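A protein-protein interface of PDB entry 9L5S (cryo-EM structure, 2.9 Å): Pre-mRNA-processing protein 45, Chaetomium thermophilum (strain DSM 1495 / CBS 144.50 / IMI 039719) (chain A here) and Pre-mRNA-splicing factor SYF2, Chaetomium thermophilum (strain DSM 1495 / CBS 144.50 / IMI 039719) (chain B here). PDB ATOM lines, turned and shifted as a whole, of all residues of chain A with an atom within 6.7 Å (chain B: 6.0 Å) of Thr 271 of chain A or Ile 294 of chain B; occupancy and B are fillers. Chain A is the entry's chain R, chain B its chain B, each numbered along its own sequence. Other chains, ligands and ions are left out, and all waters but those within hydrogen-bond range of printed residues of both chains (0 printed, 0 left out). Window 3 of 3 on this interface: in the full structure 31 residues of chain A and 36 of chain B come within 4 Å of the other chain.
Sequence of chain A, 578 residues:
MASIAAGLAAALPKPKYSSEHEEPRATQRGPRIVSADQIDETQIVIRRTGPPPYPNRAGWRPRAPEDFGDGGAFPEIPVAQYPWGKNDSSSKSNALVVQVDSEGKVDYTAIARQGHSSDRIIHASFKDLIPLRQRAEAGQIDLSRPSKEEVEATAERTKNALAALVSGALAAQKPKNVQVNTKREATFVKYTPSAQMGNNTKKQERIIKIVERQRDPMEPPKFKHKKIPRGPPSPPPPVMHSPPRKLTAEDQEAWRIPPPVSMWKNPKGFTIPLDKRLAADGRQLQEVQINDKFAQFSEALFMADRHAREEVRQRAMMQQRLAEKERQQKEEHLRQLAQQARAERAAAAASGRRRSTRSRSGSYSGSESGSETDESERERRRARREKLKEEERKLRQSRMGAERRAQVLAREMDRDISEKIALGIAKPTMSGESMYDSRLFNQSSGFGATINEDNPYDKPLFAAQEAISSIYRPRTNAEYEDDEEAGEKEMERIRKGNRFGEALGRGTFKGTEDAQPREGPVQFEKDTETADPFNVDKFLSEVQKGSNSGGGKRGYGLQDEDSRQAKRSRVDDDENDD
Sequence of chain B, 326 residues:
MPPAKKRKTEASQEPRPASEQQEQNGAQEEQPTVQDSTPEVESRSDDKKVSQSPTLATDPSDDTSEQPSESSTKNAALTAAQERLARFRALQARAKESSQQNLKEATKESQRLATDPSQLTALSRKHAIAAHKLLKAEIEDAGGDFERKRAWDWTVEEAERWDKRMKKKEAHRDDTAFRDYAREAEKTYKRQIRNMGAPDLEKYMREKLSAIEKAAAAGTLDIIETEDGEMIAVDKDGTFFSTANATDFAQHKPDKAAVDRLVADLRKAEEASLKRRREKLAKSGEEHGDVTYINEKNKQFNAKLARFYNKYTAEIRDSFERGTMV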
ATOM      1  N   ASN A 266      -4.601   0.988  19.034  1.00  0.00           N
ATOM      2  CA  ASN A 266      -5.411   1.830  18.151  1.00  0.00           C
ATOM      3  C   ASN A 266      -6.833   1.291  18.152  1.00  0.00           C
ATOM      4  O   ASN A 266      -7.223   0.522  17.266  1.00  0.00           O
ATOM      5  CB  ASN A 266      -4.840   1.864  16.732  1.00  0.00           C
ATOM      6  CG  ASN A 266      -3.567   2.679  16.629  1.00  0.00           C
ATOM      7  OD1 ASN A 266      -2.568   2.219  16.078  1.00  0.00           O
ATOM      8  ND2 ASN A 266      -3.599   3.898  17.154  1.00  0.00           N
ATOM      9  N   LYS A 268      -9.544   2.715  17.374  1.00  0.00           N
ATOM     10  CA  LYS A 268     -10.310   3.210  16.237  1.00  0.00           C
ATOM     11  C   LYS A 268      -9.560   3.046  14.919  1.00  0.00           C
ATOM     12  O   LYS A 268      -9.956   3.639  13.911  1.00  0.00           O
ATOM     13  CB  LYS A 268     -10.699   4.674  16.447  1.00  0.00           C
ATOM     14  CG  LYS A 268     -11.872   4.876  17.396  1.00  0.00           C
ATOM     15  CD  LYS A 268     -12.118   6.353  17.662  1.00  0.00           C
ATOM     16  CE  LYS A 268     -13.420   6.572  18.418  1.00  0.00           C
ATOM     17  NZ  LYS A 268     -14.610   6.228  17.592  1.00  0.00           N
ATOM     18  N   GLY A 269      -8.483   2.259  14.912  1.00  0.00           N
ATOM     19  CA  GLY A 269      -7.781   1.915  13.687  1.00  0.00           C
ATOM     20  C   GLY A 269      -7.156   3.075  12.947  1.00  0.00           C
ATOM     21  O   GLY A 269      -7.052   3.028  11.719  1.00  0.00           O
ATOM     22  N   PHE A 270      -6.740   4.119  13.656  1.00  0.00           N
ATOM     23  CA  PHE A 270      -6.208   5.305  12.998  1.00  0.00           C
ATOM     24  C   PHE A 270      -4.810   5.046  12.452  1.00  0.00           C
ATOM     25  O   PHE A 270      -3.995   4.361  13.076  1.00  0.00           O
ATOM     26  CB  PHE A 270      -6.178   6.489  13.966  1.00  0.00           C
ATOM     27  CG  PHE A 270      -7.534   7.066  14.277  1.00  0.00           C
ATOM     28  CD1 PHE A 270      -8.662   6.669  13.572  1.00  0.00           C
ATOM     29  CD2 PHE A 270      -7.677   8.016  15.276  1.00  0.00           C
ATOM     30  CE1 PHE A 270      -9.903   7.206  13.860  1.00  0.00           C
ATOM     31  CE2 PHE A 270      -8.916   8.555  15.570  1.00  0.00           C
ATOM     32  CZ  PHE A 270     -10.029   8.150  14.861  1.00  0.00           C
ATOM     33  N   THR A 271      -4.537   5.606  11.276  1.00  0.00           N
ATOM     34  CA  THR A 271      -3.211   5.542  10.669  1.00  0.00           C
ATOM     35  C   THR A 271      -2.436   6.764  11.151  1.00  0.00           C
ATOM     36  O   THR A 271      -2.471   7.828  10.527  1.00  0.00           O
ATOM     37  CB  THR A 271      -3.312   5.492   9.147  1.00  0.00           C
ATOM     38  OG1 THR A 271      -4.126   4.377   8.762  1.00  0.00           O
ATOM     39  CG2 THR A 271      -1.936   5.314   8.531  1.00  0.00           C
ATOM     40  N   ILE A 272      -1.755   6.613  12.282  1.00  0.00           N
ATOM     41  CA  ILE A 272      -0.986   7.689  12.901  1.00  0.00           C
ATOM     42  C   ILE A 272       0.305   7.850  12.107  1.00  0.00           C
ATOM     43  O   ILE A 272       0.860   6.843  11.638  1.00  0.00           O
ATOM     44  CB  ILE A 272      -0.722   7.378  14.385  1.00  0.00           C
ATOM     45  CG1 ILE A 272      -2.047   7.203  15.131  1.00  0.00           C
ATOM     46  CG2 ILE A 272       0.106   8.464  15.059  1.00  0.00           C
ATOM     47  CD1 ILE A 272      -2.929   8.433  15.114  1.00  0.00           C
ATOM     48  N   PRO A 273       0.790   9.075  11.881  1.00  0.00           N
ATOM     49  CA  PRO A 273       2.134   9.239  11.312  1.00  0.00           C
ATOM     50  C   PRO A 273       3.188   8.614  12.212  1.00  0.00           C
ATOM     51  O   PRO A 273       3.062   8.617  13.439  1.00  0.00           O
ATOM     52  CB  PRO A 273       2.305  10.760  11.225  1.00  0.00           C
ATOM     53  CG  PRO A 273       0.930  11.304  11.192  1.00  0.00           C
ATOM     54  CD  PRO A 273       0.062  10.353  11.962  1.00  0.00           C
ATOM     55  N   ARG A 277       4.411   8.503  16.440  1.00  0.00           N
ATOM     56  CA  ARG A 277       4.529   7.225  17.137  1.00  0.00           C
ATOM     57  C   ARG A 277       5.768   7.164  18.020  1.00  0.00           C
ATOM     58  O   ARG A 277       5.764   6.480  19.049  1.00  0.00           O
ATOM     59  CB  ARG A 277       4.566   6.082  16.121  1.00  0.00           C
ATOM     60  CG  ARG A 277       3.270   5.851  15.365  1.00  0.00           C
ATOM     61  CD  ARG A 277       2.387   4.845  16.078  1.00  0.00           C
ATOM     62  NE  ARG A 277       1.132   4.628  15.371  1.00  0.00           N
ATOM     63  CZ  ARG A 277       0.177   3.804  15.778  1.00  0.00           C
ATOM     64  NH1 ARG A 277       0.299   3.100  16.890  1.00  0.00           N
ATOM     65  NH2 ARG A 277      -0.928   3.682  15.048  1.00  0.00           N
ATOM     66  N   THR B 292      -2.325  11.244   5.511  1.00  0.00           N
ATOM     67  CA  THR B 292      -1.879  10.133   6.341  1.00  0.00           C
ATOM     68  C   THR B 292      -3.096   9.382   6.873  1.00  0.00           C
ATOM     69  O   THR B 292      -3.064   8.158   7.051  1.00  0.00           O
ATOM     70  CB  THR B 292      -0.991  10.645   7.480  1.00  0.00           C
ATOM     71  OG1 THR B 292       0.152  11.310   6.928  1.00  0.00           O
ATOM     72  CG2 THR B 292      -0.496   9.496   8.347  1.00  0.00           C
ATOM     73  N   TYR B 293      -4.191  10.110   7.071  1.00  0.00           N
ATOM     74  CA  TYR B 293      -5.389   9.578   7.703  1.00  0.00           C
ATOM     75  C   TYR B 293      -6.102   8.582   6.789  1.00  0.00           C
ATOM     76  O   TYR B 293      -5.721   8.354   5.639  1.00  0.00           O
ATOM     77  CB  TYR B 293      -6.323  10.723   8.090  1.00  0.00           C
ATOM     78  CG  TYR B 293      -6.857  11.535   6.920  1.00  0.00           C
ATOM     79  CD1 TYR B 293      -6.166  12.646   6.450  1.00  0.00           C
ATOM     80  CD2 TYR B 293      -8.061  11.206   6.302  1.00  0.00           C
ATOM     81  CE1 TYR B 293      -6.649  13.395   5.391  1.00  0.00           C
ATOM     82  CE2 TYR B 293      -8.549  11.947   5.243  1.00  0.00           C
ATOM     83  CZ  TYR B 293      -7.840  13.039   4.792  1.00  0.00           C
ATOM     84  OH  TYR B 293      -8.325  13.780   3.738  1.00  0.00           O
ATOM     85  N   ILE B 294      -7.154   7.971   7.333  1.00  0.00           N
ATOM     86  CA  ILE B 294      -8.089   7.175   6.541  1.00  0.00           C
ATOM     87  C   ILE B 294      -9.536   7.602   6.723  1.00  0.00           C
ATOM     88  O   ILE B 294     -10.373   7.307   5.851  1.00  0.00           O
ATOM     89  CB  ILE B 294      -7.937   5.668   6.855  1.00  0.00           C
ATOM     90  CG1 ILE B 294      -8.241   5.388   8.329  1.00  0.00           C
ATOM     91  CG2 ILE B 294      -6.552   5.158   6.472  1.00  0.00           C
ATOM     92  CD1 ILE B 294      -8.406   3.917   8.648  1.00  0.00           C
ATOM     93  N   ASN B 295      -9.886   8.301   7.803  1.00  0.00           N
ATOM     94  CA  ASN B 295     -11.249   8.730   8.092  1.00  0.00           C
ATOM     95  C   ASN B 295     -11.249  10.219   8.423  1.00  0.00           C
ATOM     96  O   ASN B 295     -10.195  10.845   8.573  1.00  0.00           O
ATOM     97  CB  ASN B 295     -11.853   7.925   9.251  1.00  0.00           C
ATOM     98  CG  ASN B 295     -12.253   6.519   8.847  1.00  0.00           C
ATOM     99  OD1 ASN B 295     -12.243   6.171   7.668  1.00  0.00           O
ATOM    100  ND2 ASN B 295     -12.605   5.701   9.831  1.00  0.00           N
ATOM    101  N   GLU B 296     -12.452  10.787   8.550  1.00  0.00           N
ATOM    102  CA  GLU B 296     -12.577  12.201   8.898  1.00  0.00           C
ATOM    103  C   GLU B 296     -12.130  12.463  10.332  1.00  0.00           C
ATOM    104  O   GLU B 296     -11.406  13.434  10.596  1.00  0.00           O
ATOM    105  CB  GLU B 296     -14.019  12.663   8.689  1.00  0.00           C
ATOM    106  CG  GLU B 296     -14.286  14.105   9.091  1.00  0.00           C
ATOM    107  CD  GLU B 296     -15.032  14.212  10.407  1.00  0.00           C
ATOM    108  OE1 GLU B 296     -15.529  13.174  10.895  1.00  0.00           O
ATOM    109  OE2 GLU B 296     -15.125  15.330  10.954  1.00  0.00           O
ATOM    110  N   ASN B 298     -10.081  10.561  11.933  1.00  0.00           N
ATOM    111  CA  ASN B 298      -8.639  10.354  11.847  1.00  0.00           C
ATOM    112  C   ASN B 298      -7.934  11.606  11.340  1.00  0.00           C
ATOM    113  O   ASN B 298      -6.861  11.963  11.836  1.00  0.00           O
ATOM    114  CB  ASN B 298      -8.341   9.162  10.937  1.00  0.00           C
ATOM    115  CG  ASN B 298      -6.925   8.638  11.096  1.00  0.00           C
ATOM    116  OD1 ASN B 298      -6.138   9.152  11.891  1.00  0.00           O
ATOM    117  ND2 ASN B 298      -6.595   7.608  10.330  1.00  0.00           N
ATOM    118  N   LYS B 299      -8.528  12.284  10.352  1.00  0.00           N
ATOM    119  CA  LYS B 299      -7.953  13.524   9.834  1.00  0.00           C
ATOM    120  C   LYS B 299      -7.916  14.610  10.901  1.00  0.00           C
ATOM    121  O   LYS B 299      -6.908  15.313  11.048  1.00  0.00           O
ATOM    122  CB  LYS B 299      -8.750  13.995   8.617  1.00  0.00           C
ATOM    123  CG  LYS B 299      -8.268  15.305   8.018  1.00  0.00           C
ATOM    124  CD  LYS B 299      -9.135  15.720   6.840  1.00  0.00           C
ATOM    125  CE  LYS B 299      -8.479  16.826   6.032  1.00  0.00           C
ATOM    126  NZ  LYS B 299      -8.949  16.831   4.619  1.00  0.00           N
ATOM    127  N   ASN B 302      -5.261  13.693  13.504  1.00  0.00           N
ATOM    128  CA  ASN B 302      -3.915  13.926  12.992  1.00  0.00           C
ATOM    129  C   ASN B 302      -3.600  15.414  12.894  1.00  0.00           C
ATOM    130  O   ASN B 302      -2.450  15.816  13.106  1.00  0.00           O
ATOM    131  CB  ASN B 302      -3.744  13.249  11.634  1.00  0.00           C
ATOM    132  CG  ASN B 302      -3.746  11.740  11.739  1.00  0.00           C
ATOM    133  OD1 ASN B 302      -3.033  11.163  12.556  1.00  0.00           O
ATOM    134  ND2 ASN B 302      -4.557  11.091  10.914  1.00  0.00           N
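N of Thr 271 of chain A sits close to ND2 of Asn 298 of chain B, 3.0 Å away.
ND2 of Asn 298 of chain B sits close to N of Ile 294 of chain B. The side-chain amide nitrogen (ND2) of Asn 302 of chain B lies within hydrogen-bond range of the backbone carbonyl oxygen (O) of Asn 298 of chain B (2.6 Å).
O of Gly 269 of chain A touches CD1 of Ile 294 of chain B, 3.5 Å away. CB of Phe 270 of chain A touches OD1 of Asn 298 of chain B, at 3.4 Å. Thr 292 of chain B touches Thr 271 of chain A. OG1 of Thr 271 of chain A touches CG2 of Ile 294 of chain B (3.4 Å). Asn 302 of chain B touches Thr 271 of chain A (ND2 to O, 3.9 Å). Asn 302 of chain B touches Ile 272 of chain A. Pro 273 of chain A touches Thr 292 of chain B. CD of Pro 273 of chain A touches OD1 of Asn 302 of chain B, 3.3 Å away.
Of the printed residues of chain B, Gly 269 of chain A touches Ile 294. Of chain B, only Thr 292 (3.4 Å), Ile 294 (3.4 Å), Asn 298 (3.0 Å) and Asn 302 (3.9 Å) come within 4 Å of Thr 271 of chain A. Of the printed residues of chain B, Pro 273 of chain A touches Thr 292 and Asn 302. Of chain A, only Gly 269 (3.5 Å) and Thr 271 (3.4 Å) come within 4 Å of Ile 294 of chain B. The nearest residue of chain B that does not touch Thr 271 of chain A is Tyr 293 of chain B (4.4 Å). The nearest printed residue of chain A that does not touch Asn 298 of chain B is Ile 272 of chain A (4.6 Å).
Printed residues of chain B that touch a printed residue of chain A: Thr 292, Ile 294, Asn 298 and Asn 302. Hydrophobic or aromatic side chains of chain A that line the printed part of chain B: Phe 270, Ile 272 and Pro 273. Along chain A the printed residues that touch a printed residue of chain B span positions 269 to 273. Among the printed residues, no Asp or Glu carboxylate lies within 4 Å of a Lys or Arg side-chain nitrogen of the other chain.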
